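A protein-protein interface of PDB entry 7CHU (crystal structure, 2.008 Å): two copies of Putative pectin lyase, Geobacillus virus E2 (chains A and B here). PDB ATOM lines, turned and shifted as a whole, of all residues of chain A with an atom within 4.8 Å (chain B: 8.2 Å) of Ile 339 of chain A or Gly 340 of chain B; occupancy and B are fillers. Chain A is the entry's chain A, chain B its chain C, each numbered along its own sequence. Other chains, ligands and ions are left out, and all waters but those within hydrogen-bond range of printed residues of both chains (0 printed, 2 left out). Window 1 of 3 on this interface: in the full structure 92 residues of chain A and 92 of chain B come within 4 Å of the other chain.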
ATOM      1  N   TYR A 315     -13.716  17.334  22.847  1.00  0.00           N
ATOM      2  CA  TYR A 315     -14.772  17.876  21.997  1.00  0.00           C
ATOM      3  C   TYR A 315     -16.064  17.151  22.350  1.00  0.00           C
ATOM      4  O   TYR A 315     -16.190  15.949  22.095  1.00  0.00           O
ATOM      5  CB  TYR A 315     -14.451  17.686  20.515  1.00  0.00           C
ATOM      6  CG  TYR A 315     -13.097  18.197  20.041  1.00  0.00           C
ATOM      7  CD1 TYR A 315     -11.924  17.564  20.432  1.00  0.00           C
ATOM      8  CD2 TYR A 315     -13.001  19.283  19.159  1.00  0.00           C
ATOM      9  CE1 TYR A 315     -10.694  17.988  19.971  1.00  0.00           C
ATOM     10  CE2 TYR A 315     -11.774  19.724  18.690  1.00  0.00           C
ATOM     11  CZ  TYR A 315     -10.615  19.062  19.107  1.00  0.00           C
ATOM     12  OH  TYR A 315      -9.384  19.464  18.645  1.00  0.00           O
ATOM     13  N   VAL A 316     -17.005  17.859  22.958  1.00  0.00           N
ATOM     14  CA  VAL A 316     -18.304  17.278  23.273  1.00  0.00           C
ATOM     15  C   VAL A 316     -19.316  17.946  22.343  1.00  0.00           C
ATOM     16  O   VAL A 316     -19.846  19.028  22.643  1.00  0.00           O
ATOM     17  CB  VAL A 316     -18.663  17.454  24.759  1.00  0.00           C
ATOM     18  CG1 VAL A 316     -19.945  16.721  25.099  1.00  0.00           C
ATOM     19  CG2 VAL A 316     -17.485  16.971  25.670  1.00  0.00           C
ATOM     20  N   MET A 317     -19.578  17.296  21.206  1.00  0.00           N
ATOM     21  CA  MET A 317     -20.321  17.869  20.094  1.00  0.00           C
ATOM     22  C   MET A 317     -21.717  17.270  20.011  1.00  0.00           C
ATOM     23  O   MET A 317     -21.871  16.051  19.862  1.00  0.00           O
ATOM     24  CB  MET A 317     -19.585  17.651  18.772  1.00  0.00           C
ATOM     25  CG  MET A 317     -18.124  18.061  18.797  1.00  0.00           C
ATOM     26  SD  MET A 317     -17.885  19.837  19.061  1.00  0.00           S
ATOM     27  CE  MET A 317     -18.655  20.522  17.585  1.00  0.00           C
ATOM     28  N   ASN A 318     -22.722  18.141  20.055  1.00  0.00           N
ATOM     29  CA  ASN A 318     -24.134  17.776  19.910  1.00  0.00           C
ATOM     30  C   ASN A 318     -24.456  16.496  20.689  1.00  0.00           C
ATOM     31  O   ASN A 318     -24.954  15.500  20.161  1.00  0.00           O
ATOM     32  CB  ASN A 318     -24.559  17.679  18.420  1.00  0.00           C
ATOM     33  CG  ASN A 318     -23.504  17.033  17.505  1.00  0.00           C
ATOM     34  OD1 ASN A 318     -22.448  17.623  17.205  1.00  0.00           O
ATOM     35  ND2 ASN A 318     -23.809  15.832  17.020  1.00  0.00           N
ATOM     36  N   LYS A 337     -14.427  21.714  24.661  1.00  0.00           N
ATOM     37  CA  LYS A 337     -15.449  22.337  23.825  1.00  0.00           C
ATOM     38  C   LYS A 337     -16.769  21.602  24.005  1.00  0.00           C
ATOM     39  O   LYS A 337     -16.870  20.403  23.708  1.00  0.00           O
ATOM     40  CB  LYS A 337     -15.009  22.333  22.361  1.00  0.00           C
ATOM     41  CG  LYS A 337     -13.776  23.211  22.164  1.00  0.00           C
ATOM     42  CD  LYS A 337     -13.101  22.979  20.839  1.00  0.00           C
ATOM     43  CE  LYS A 337     -11.826  23.850  20.712  1.00  0.00           C
ATOM     44  NZ  LYS A 337     -10.829  23.602  21.811  1.00  0.00           N
ATOM     45  N   ILE A 338     -17.764  22.324  24.503  1.00  0.00           N
ATOM     46  CA  ILE A 338     -19.116  21.837  24.741  1.00  0.00           C
ATOM     47  C   ILE A 338     -19.993  22.615  23.766  1.00  0.00           C
ATOM     48  O   ILE A 338     -20.315  23.789  23.991  1.00  0.00           O
ATOM     49  CB  ILE A 338     -19.567  22.044  26.197  1.00  0.00           C
ATOM     50  CG1 ILE A 338     -18.444  21.723  27.220  1.00  0.00           C
ATOM     51  CG2 ILE A 338     -20.869  21.269  26.492  1.00  0.00           C
ATOM     52  CD1 ILE A 338     -18.093  20.292  27.271  1.00  0.00           C
ATOM     53  N   ILE A 339     -20.330  21.999  22.638  1.00  0.00           N
ATOM     54  CA  ILE A 339     -20.920  22.714  21.507  1.00  0.00           C
ATOM     55  C   ILE A 339     -22.194  22.004  21.081  1.00  0.00           C
ATOM     56  O   ILE A 339     -22.158  20.816  20.728  1.00  0.00           O
ATOM     57  CB  ILE A 339     -19.935  22.808  20.325  1.00  0.00           C
ATOM     58  CG1 ILE A 339     -18.768  23.745  20.669  1.00  0.00           C
ATOM     59  CG2 ILE A 339     -20.661  23.255  19.048  1.00  0.00           C
ATOM     60  CD1 ILE A 339     -17.758  23.875  19.550  1.00  0.00           C
ATOM     61  N   GLY A 340     -23.307  22.742  21.061  1.00  0.00           N
ATOM     62  CA  GLY A 340     -24.562  22.194  20.590  1.00  0.00           C
ATOM     63  C   GLY A 340     -25.150  21.112  21.466  1.00  0.00           C
ATOM     64  O   GLY A 340     -25.925  20.292  20.976  1.00  0.00           O
ATOM     65  N   CYS A 341     -24.803  21.070  22.750  1.00  0.00           N
ATOM     66  CA  CYS A 341     -25.344  20.020  23.595  1.00  0.00           C
ATOM     67  C   CYS A 341     -26.642  20.479  24.241  1.00  0.00           C
ATOM     68  O   CYS A 341     -26.895  21.673  24.413  1.00  0.00           O
ATOM     69  CB  CYS A 341     -24.331  19.610  24.681  1.00  0.00           C
ATOM     70  SG  CYS A 341     -22.760  19.034  23.955  1.00  0.00           S
ATOM     71  N   ASP A 363     -20.856  26.580  23.757  1.00  0.00           N
ATOM     72  CA  ASP A 363     -21.332  27.307  22.590  1.00  0.00           C
ATOM     73  C   ASP A 363     -22.524  26.613  21.932  1.00  0.00           C
ATOM     74  O   ASP A 363     -22.484  25.406  21.669  1.00  0.00           O
ATOM     75  CB  ASP A 363     -20.193  27.476  21.583  1.00  0.00           C
ATOM     76  CG  ASP A 363     -20.622  28.252  20.357  1.00  0.00           C
ATOM     77  OD1 ASP A 363     -20.477  27.731  19.231  1.00  0.00           O
ATOM     78  OD2 ASP A 363     -21.130  29.389  20.518  1.00  0.00           O
ATOM     79  N   CYS A 365     -25.359  25.803  23.135  1.00  0.00           N
ATOM     80  CA  CYS A 365     -26.004  24.811  23.987  1.00  0.00           C
ATOM     81  C   CYS A 365     -27.311  25.359  24.528  1.00  0.00           C
ATOM     82  O   CYS A 365     -27.558  26.565  24.503  1.00  0.00           O
ATOM     83  CB  CYS A 365     -25.107  24.409  25.169  1.00  0.00           C
ATOM     84  SG  CYS A 365     -23.555  23.600  24.702  1.00  0.00           S
ATOM     85  N   GLY B 286     -14.303  15.764  12.848  1.00  0.00           N
ATOM     86  CA  GLY B 286     -13.479  15.022  13.793  1.00  0.00           C
ATOM     87  C   GLY B 286     -12.136  14.604  13.250  1.00  0.00           C
ATOM     88  O   GLY B 286     -11.567  13.616  13.722  1.00  0.00           O
ATOM     89  N   VAL B 316     -15.496  22.492   8.443  1.00  0.00           N
ATOM     90  CA  VAL B 316     -14.375  21.951   9.212  1.00  0.00           C
ATOM     91  C   VAL B 316     -14.801  21.883  10.672  1.00  0.00           C
ATOM     92  O   VAL B 316     -14.712  22.879  11.408  1.00  0.00           O
ATOM     93  CB  VAL B 316     -13.114  22.812   9.013  1.00  0.00           C
ATOM     94  CG1 VAL B 316     -11.895  22.155   9.689  1.00  0.00           C
ATOM     95  CG2 VAL B 316     -12.839  23.015   7.534  1.00  0.00           C
ATOM     96  N   MET B 317     -15.338  20.732  11.079  1.00  0.00           N
ATOM     97  CA  MET B 317     -16.073  20.585  12.333  1.00  0.00           C
ATOM     98  C   MET B 317     -15.253  19.772  13.326  1.00  0.00           C
ATOM     99  O   MET B 317     -14.913  18.620  13.050  1.00  0.00           O
ATOM    100  CB  MET B 317     -17.412  19.873  12.122  1.00  0.00           C
ATOM    101  CG  MET B 317     -18.264  20.420  10.997  1.00  0.00           C
ATOM    102  SD  MET B 317     -18.946  22.024  11.525  1.00  0.00           S
ATOM    103  CE  MET B 317     -17.839  23.092  10.760  1.00  0.00           C
ATOM    104  N   ASN B 318     -15.020  20.344  14.499  1.00  0.00           N
ATOM    105  CA  ASN B 318     -14.276  19.700  15.600  1.00  0.00           C
ATOM    106  C   ASN B 318     -13.058  18.931  15.084  1.00  0.00           C
ATOM    107  O   ASN B 318     -12.862  17.737  15.337  1.00  0.00           O
ATOM    108  CB  ASN B 318     -15.200  18.822  16.473  1.00  0.00           C
ATOM    109  CG  ASN B 318     -16.226  18.021  15.677  1.00  0.00           C
ATOM    110  OD1 ASN B 318     -17.222  18.573  15.179  1.00  0.00           O
ATOM    111  ND2 ASN B 318     -16.000  16.698  15.567  1.00  0.00           N
ATOM    112  N   CYS B 319     -12.230  19.648  14.325  1.00  0.00           N
ATOM    113  CA  CYS B 319     -10.976  19.085  13.845  1.00  0.00           C
ATOM    114  C   CYS B 319      -9.799  19.572  14.687  1.00  0.00           C
ATOM    115  O   CYS B 319      -9.833  20.640  15.306  1.00  0.00           O
ATOM    116  CB  CYS B 319     -10.748  19.428  12.368  1.00  0.00           C
ATOM    117  SG  CYS B 319     -11.938  18.639  11.250  1.00  0.00           S
ATOM    118  N   TYR B 320      -8.751  18.759  14.705  1.00  0.00           N
ATOM    119  CA  TYR B 320      -7.574  18.979  15.544  1.00  0.00           C
ATOM    120  C   TYR B 320      -6.395  19.309  14.642  1.00  0.00           C
ATOM    121  O   TYR B 320      -6.064  18.530  13.739  1.00  0.00           O
ATOM    122  CB  TYR B 320      -7.286  17.727  16.373  1.00  0.00           C
ATOM    123  CG  TYR B 320      -5.864  17.530  16.889  1.00  0.00           C
ATOM    124  CD1 TYR B 320      -5.247  18.463  17.726  1.00  0.00           C
ATOM    125  CD2 TYR B 320      -5.179  16.367  16.601  1.00  0.00           C
ATOM    126  CE1 TYR B 320      -3.941  18.249  18.217  1.00  0.00           C
ATOM    127  CE2 TYR B 320      -3.903  16.143  17.089  1.00  0.00           C
ATOM    128  CZ  TYR B 320      -3.297  17.077  17.894  1.00  0.00           C
ATOM    129  OH  TYR B 320      -2.034  16.831  18.336  1.00  0.00           O
ATOM    130  N   PHE B 321      -5.769  20.453  14.881  1.00  0.00           N
ATOM    131  CA  PHE B 321      -4.605  20.891  14.121  1.00  0.00           C
ATOM    132  C   PHE B 321      -3.398  21.019  15.041  1.00  0.00           C
ATOM    133  O   PHE B 321      -3.476  21.707  16.071  1.00  0.00           O
ATOM    134  CB  PHE B 321      -4.897  22.246  13.461  1.00  0.00           C
ATOM    135  CG  PHE B 321      -5.897  22.168  12.356  1.00  0.00           C
ATOM    136  CD1 PHE B 321      -7.261  22.218  12.623  1.00  0.00           C
ATOM    137  CD2 PHE B 321      -5.475  22.026  11.045  1.00  0.00           C
ATOM    138  CE1 PHE B 321      -8.180  22.154  11.592  1.00  0.00           C
ATOM    139  CE2 PHE B 321      -6.403  21.963   9.988  1.00  0.00           C
ATOM    140  CZ  PHE B 321      -7.740  22.006  10.262  1.00  0.00           C
ATOM    141  N   LYS B 337     -16.681  27.103   7.037  1.00  0.00           N
ATOM    142  CA  LYS B 337     -17.123  27.043   8.417  1.00  0.00           C
ATOM    143  C   LYS B 337     -16.087  26.302   9.235  1.00  0.00           C
ATOM    144  O   LYS B 337     -15.827  25.119   8.979  1.00  0.00           O
ATOM    145  CB  LYS B 337     -18.482  26.370   8.514  1.00  0.00           C
ATOM    146  CG  LYS B 337     -19.566  27.214   7.861  1.00  0.00           C
ATOM    147  CD  LYS B 337     -20.777  26.380   7.570  1.00  0.00           C
ATOM    148  CE  LYS B 337     -21.912  27.285   7.035  1.00  0.00           C
ATOM    149  NZ  LYS B 337     -21.434  28.038   5.840  1.00  0.00           N
ATOM    150  N   ILE B 338     -15.485  27.008  10.186  1.00  0.00           N
ATOM    151  CA  ILE B 338     -14.466  26.465  11.081  1.00  0.00           C
ATOM    152  C   ILE B 338     -15.075  26.518  12.474  1.00  0.00           C
ATOM    153  O   ILE B 338     -15.090  27.579  13.121  1.00  0.00           O
ATOM    154  CB  ILE B 338     -13.143  27.247  11.021  1.00  0.00           C
ATOM    155  CG1 ILE B 338     -12.733  27.586   9.583  1.00  0.00           C
ATOM    156  CG2 ILE B 338     -12.007  26.535  11.865  1.00  0.00           C
ATOM    157  CD1 ILE B 338     -12.488  26.416   8.743  1.00  0.00           C
ATOM    158  N   ILE B 339     -15.585  25.383  12.942  1.00  0.00           N
ATOM    159  CA  ILE B 339     -16.425  25.335  14.133  1.00  0.00           C
ATOM    160  C   ILE B 339     -15.857  24.322  15.124  1.00  0.00           C
ATOM    161  O   ILE B 339     -15.730  23.136  14.799  1.00  0.00           O
ATOM    162  CB  ILE B 339     -17.871  24.987  13.773  1.00  0.00           C
ATOM    163  CG1 ILE B 339     -18.453  26.114  12.897  1.00  0.00           C
ATOM    164  CG2 ILE B 339     -18.695  24.773  15.052  1.00  0.00           C
ATOM    165  CD1 ILE B 339     -19.857  25.836  12.373  1.00  0.00           C
ATOM    166  N   GLY B 340     -15.529  24.786  16.328  1.00  0.00           N
ATOM    167  CA  GLY B 340     -15.084  23.891  17.378  1.00  0.00           C
ATOM    168  C   GLY B 340     -13.750  23.244  17.096  1.00  0.00           C
ATOM    169  O   GLY B 340     -13.508  22.125  17.539  1.00  0.00           O
ATOM    170  N   CYS B 341     -12.877  23.916  16.369  1.00  0.00           N
ATOM    171  CA  CYS B 341     -11.562  23.341  16.123  1.00  0.00           C
ATOM    172  C   CYS B 341     -10.562  23.852  17.156  1.00  0.00           C
ATOM    173  O   CYS B 341     -10.748  24.907  17.773  1.00  0.00           O
ATOM    174  CB  CYS B 341     -11.091  23.641  14.694  1.00  0.00           C
ATOM    175  SG  CYS B 341     -12.153  23.015  13.323  1.00  0.00           S
ATOM    176  N   ASP B 342      -9.488  23.080  17.349  1.00  0.00           N
ATOM    177  CA  ASP B 342      -8.373  23.491  18.191  1.00  0.00           C
ATOM    178  C   ASP B 342      -7.066  23.492  17.404  1.00  0.00           C
ATOM    179  O   ASP B 342      -6.793  22.585  16.610  1.00  0.00           O
ATOM    180  CB  ASP B 342      -8.241  22.601  19.418  1.00  0.00           C
ATOM    181  CG  ASP B 342      -7.452  23.273  20.533  1.00  0.00           C
ATOM    182  OD1 ASP B 342      -8.072  23.975  21.369  1.00  0.00           O
ATOM    183  OD2 ASP B 342      -6.208  23.108  20.546  1.00  0.00           O
ATOM    184  N   PHE B 343      -6.281  24.541  17.610  1.00  0.00           N
ATOM    185  CA  PHE B 343      -5.084  24.816  16.831  1.00  0.00           C
ATOM    186  C   PHE B 343      -3.920  24.937  17.808  1.00  0.00           C
ATOM    187  O   PHE B 343      -4.025  25.667  18.794  1.00  0.00           O
ATOM    188  CB  PHE B 343      -5.253  26.117  16.005  1.00  0.00           C
ATOM    189  CG  PHE B 343      -6.440  26.095  15.025  1.00  0.00           C
ATOM    190  CD1 PHE B 343      -6.276  25.596  13.724  1.00  0.00           C
ATOM    191  CD2 PHE B 343      -7.695  26.573  15.399  1.00  0.00           C
ATOM    192  CE1 PHE B 343      -7.341  25.579  12.824  1.00  0.00           C
ATOM    193  CE2 PHE B 343      -8.772  26.557  14.513  1.00  0.00           C
ATOM    194  CZ  PHE B 343      -8.597  26.055  13.219  1.00  0.00           C
ATOM    195  N   VAL B 361     -16.616  31.707   8.721  1.00  0.00           N
ATOM    196  CA  VAL B 361     -16.933  31.825  10.135  1.00  0.00           C
ATOM    197  C   VAL B 361     -15.993  30.943  10.959  1.00  0.00           C
ATOM    198  O   VAL B 361     -15.717  29.791  10.593  1.00  0.00           O
ATOM    199  CB  VAL B 361     -18.413  31.485  10.402  1.00  0.00           C
ATOM    200  CG1 VAL B 361     -18.778  30.194   9.762  1.00  0.00           C
ATOM    201  CG2 VAL B 361     -18.698  31.440  11.898  1.00  0.00           C
ATOM    202  N   ILE B 362     -15.502  31.493  12.069  1.00  0.00           N
ATOM    203  CA  ILE B 362     -14.636  30.804  13.016  1.00  0.00           C
ATOM    204  C   ILE B 362     -15.381  30.809  14.340  1.00  0.00           C
ATOM    205  O   ILE B 362     -15.467  31.845  15.018  1.00  0.00           O
ATOM    206  CB  ILE B 362     -13.268  31.483  13.135  1.00  0.00           C
ATOM    207  CG1 ILE B 362     -12.589  31.523  11.759  1.00  0.00           C
ATOM    208  CG2 ILE B 362     -12.413  30.802  14.198  1.00  0.00           C
ATOM    209  CD1 ILE B 362     -11.398  32.490  11.682  1.00  0.00           C
ATOM    210  N   ASP B 363     -15.959  29.676  14.707  1.00  0.00           N
ATOM    211  CA  ASP B 363     -16.927  29.633  15.800  1.00  0.00           C
ATOM    212  C   ASP B 363     -16.568  28.543  16.803  1.00  0.00           C
ATOM    213  O   ASP B 363     -16.332  27.396  16.411  1.00  0.00           O
ATOM    214  CB  ASP B 363     -18.326  29.382  15.242  1.00  0.00           C
ATOM    215  CG  ASP B 363     -19.403  29.967  16.108  1.00  0.00           C
ATOM    216  OD1 ASP B 363     -19.466  29.579  17.290  1.00  0.00           O
ATOM    217  OD2 ASP B 363     -20.186  30.823  15.609  1.00  0.00           O
ATOM    218  N   GLY B 364     -16.566  28.885  18.090  1.00  0.00           N
ATOM    219  CA  GLY B 364     -16.317  27.897  19.123  1.00  0.00           C
ATOM    220  C   GLY B 364     -14.929  27.305  19.127  1.00  0.00           C
ATOM    221  O   GLY B 364     -14.720  26.235  19.715  1.00  0.00           O
ATOM    222  N   CYS B 365     -13.969  27.969  18.495  1.00  0.00           N
ATOM    223  CA  CYS B 365     -12.630  27.434  18.316  1.00  0.00           C
ATOM    224  C   CYS B 365     -11.724  27.909  19.448  1.00  0.00           C
ATOM    225  O   CYS B 365     -12.008  28.907  20.116  1.00  0.00           O
ATOM    226  CB  CYS B 365     -12.057  27.900  16.970  1.00  0.00           C
ATOM    227  SG  CYS B 365     -12.854  27.157  15.557  1.00  0.00           S
ATOM    228  N   SER B 366     -10.588  27.223  19.619  1.00  0.00           N
ATOM    229  CA  SER B 366      -9.548  27.732  20.510  1.00  0.00           C
ATOM    230  C   SER B 366      -8.191  27.253  20.023  1.00  0.00           C
ATOM    231  O   SER B 366      -8.063  26.631  18.962  1.00  0.00           O
ATOM    232  CB  SER B 366      -9.780  27.329  21.967  1.00  0.00           C
ATOM    233  OG  SER B 366      -9.082  28.228  22.847  1.00  0.00           O
ATOM    234  N   CYS B 387     -16.587  34.019  16.450  1.00  0.00           N
ATOM    235  CA  CYS B 387     -17.071  33.978  17.831  1.00  0.00           C
ATOM    236  C   CYS B 387     -16.283  32.871  18.552  1.00  0.00           C
ATOM    237  O   CYS B 387     -16.723  31.721  18.633  1.00  0.00           O
ATOM    238  CB  CYS B 387     -18.576  33.717  17.903  1.00  0.00           C
ATOM    239  SG  CYS B 387     -19.227  33.715  19.596  1.00  0.00           S
ATOM    240  N   SER B 388     -15.098  33.222  19.052  1.00  0.00           N
ATOM    241  CA  SER B 388     -14.197  32.240  19.656  1.00  0.00           C
ATOM    242  C   SER B 388     -13.298  32.920  20.664  1.00  0.00           C
ATOM    243  O   SER B 388     -13.112  34.141  20.642  1.00  0.00           O
ATOM    244  CB  SER B 388     -13.312  31.524  18.616  1.00  0.00           C
ATOM    245  OG  SER B 388     -14.096  30.814  17.680  1.00  0.00           O
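Met 317 of chain A touches Asn 318 of chain B, but with the chains exchanged Asn 318 of chain A does not touch Met 317 of chain B (7.5 Å).
Lys 337 of chain A touches Cys 341 of chain B, but with the chains exchanged Cys 341 of chain A does not touch Lys 337 of chain B (16.5 Å).
Ile 339 of chain A touches Gly 340 of chain B, but with the chains exchanged Gly 340 of chain A does not touch Ile 339 of chain B (7.8 Å).
Asp 363 of chain A touches its own counterpart, Asp 363 of chain B.
Positions printed for both chains: 316, 317, 318, 337, 338, 339, 340, 341, 363 and 365.
Along chain B the printed residues that touch a printed residue of chain A span positions 318 to 366.
Among the printed residues, 14 pairs touch across the chains.
CB of Asn 318 of chain B touches CD2 of Tyr 315 of chain A, 3.5 Å away.
O of Cys 319 of chain B touches OH of Tyr 315 of chain A (3.6 Å).
Tyr 320 of chain B touches Tyr 315 of chain A.
Tyr 315 of chain A touches Gly 340 of chain B (CE2 to O, 3.2 Å).
Tyr 315 of chain A touches Asp 342 of chain B.
O of Cys 341 of chain B touches CE of Lys 337 of chain A, at 3.3 Å.
Lys 337 of chain A touches Gly 364 of chain B.
Ser 366 of chain B touches Lys 337 of chain A.
Gly 340 of chain B touches Ile 339 of chain A.
CD1 of Ile 339 of chain A touches O of Gly 364 of chain B, at 3.9 Å.
The backbone carbonyl oxygen (O) of Lys 337 of chain A sits at hydrogen-bond distance from the backbone NH (N) of Val 316 of chain A, at 2.7 Å.
N of Asp 363 of chain A lies within hydrogen-bond range of O of Ile 338 of chain A, at 2.9 Å.
The backbone carbonyl oxygen (O) of Met 317 of chain B is in hydrogen-bond range of the side-chain sulfur (SG) of Cys 319 of chain B (3.5 Å).
The backbone NH (N) of Phe 321 of chain B sits at hydrogen-bond distance from the backbone carbonyl oxygen (O) of Asp 342 of chain B.
The backbone NH (N) of Gly 340 of chain B is in hydrogen-bond range of the backbone carbonyl oxygen (O) of Asp 363 of chain B (2.7 Å).
O of Cys 341 of chain B lies within hydrogen-bond range of N of Ser 366 of chain B (3.0 Å).
Of chain B, only Gly 340 (3.4 Å) and Gly 364 (3.9 Å) come within 4 Å of Ile 339 of chain A.
No residue of chain B comes within 4 Å of Gly 340 of chain A.
Of the printed residues of chain A, Tyr 320 of chain B touches Tyr 315 (3.5 Å).
Printed residues of chain A within 4 Å of Asp 363 of chain B: Asp 363.
Printed residues of chain A within 4 Å of Cys 319 of chain B: Tyr 315 (3.6 Å).
Of the printed residues of chain A, Asn 318 of chain B touches Tyr 315 and Met 317.
Printed residues of chain A within 4 Å of Asp 342 of chain B: Tyr 315 and Lys 337.
The nearest residue of chain B that does not touch Ile 339 of chain A is Ile 339 of chain B (4.7 Å).
The side-chain carboxylate (OD1) of Asp 342 of chain B lies within salt-bridge range of the side-chain amino group (NZ) of Lys 337 of chain A.
OD1 of Asp 363 of chain A sits close to OD1 of Asp 363 of chain B.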
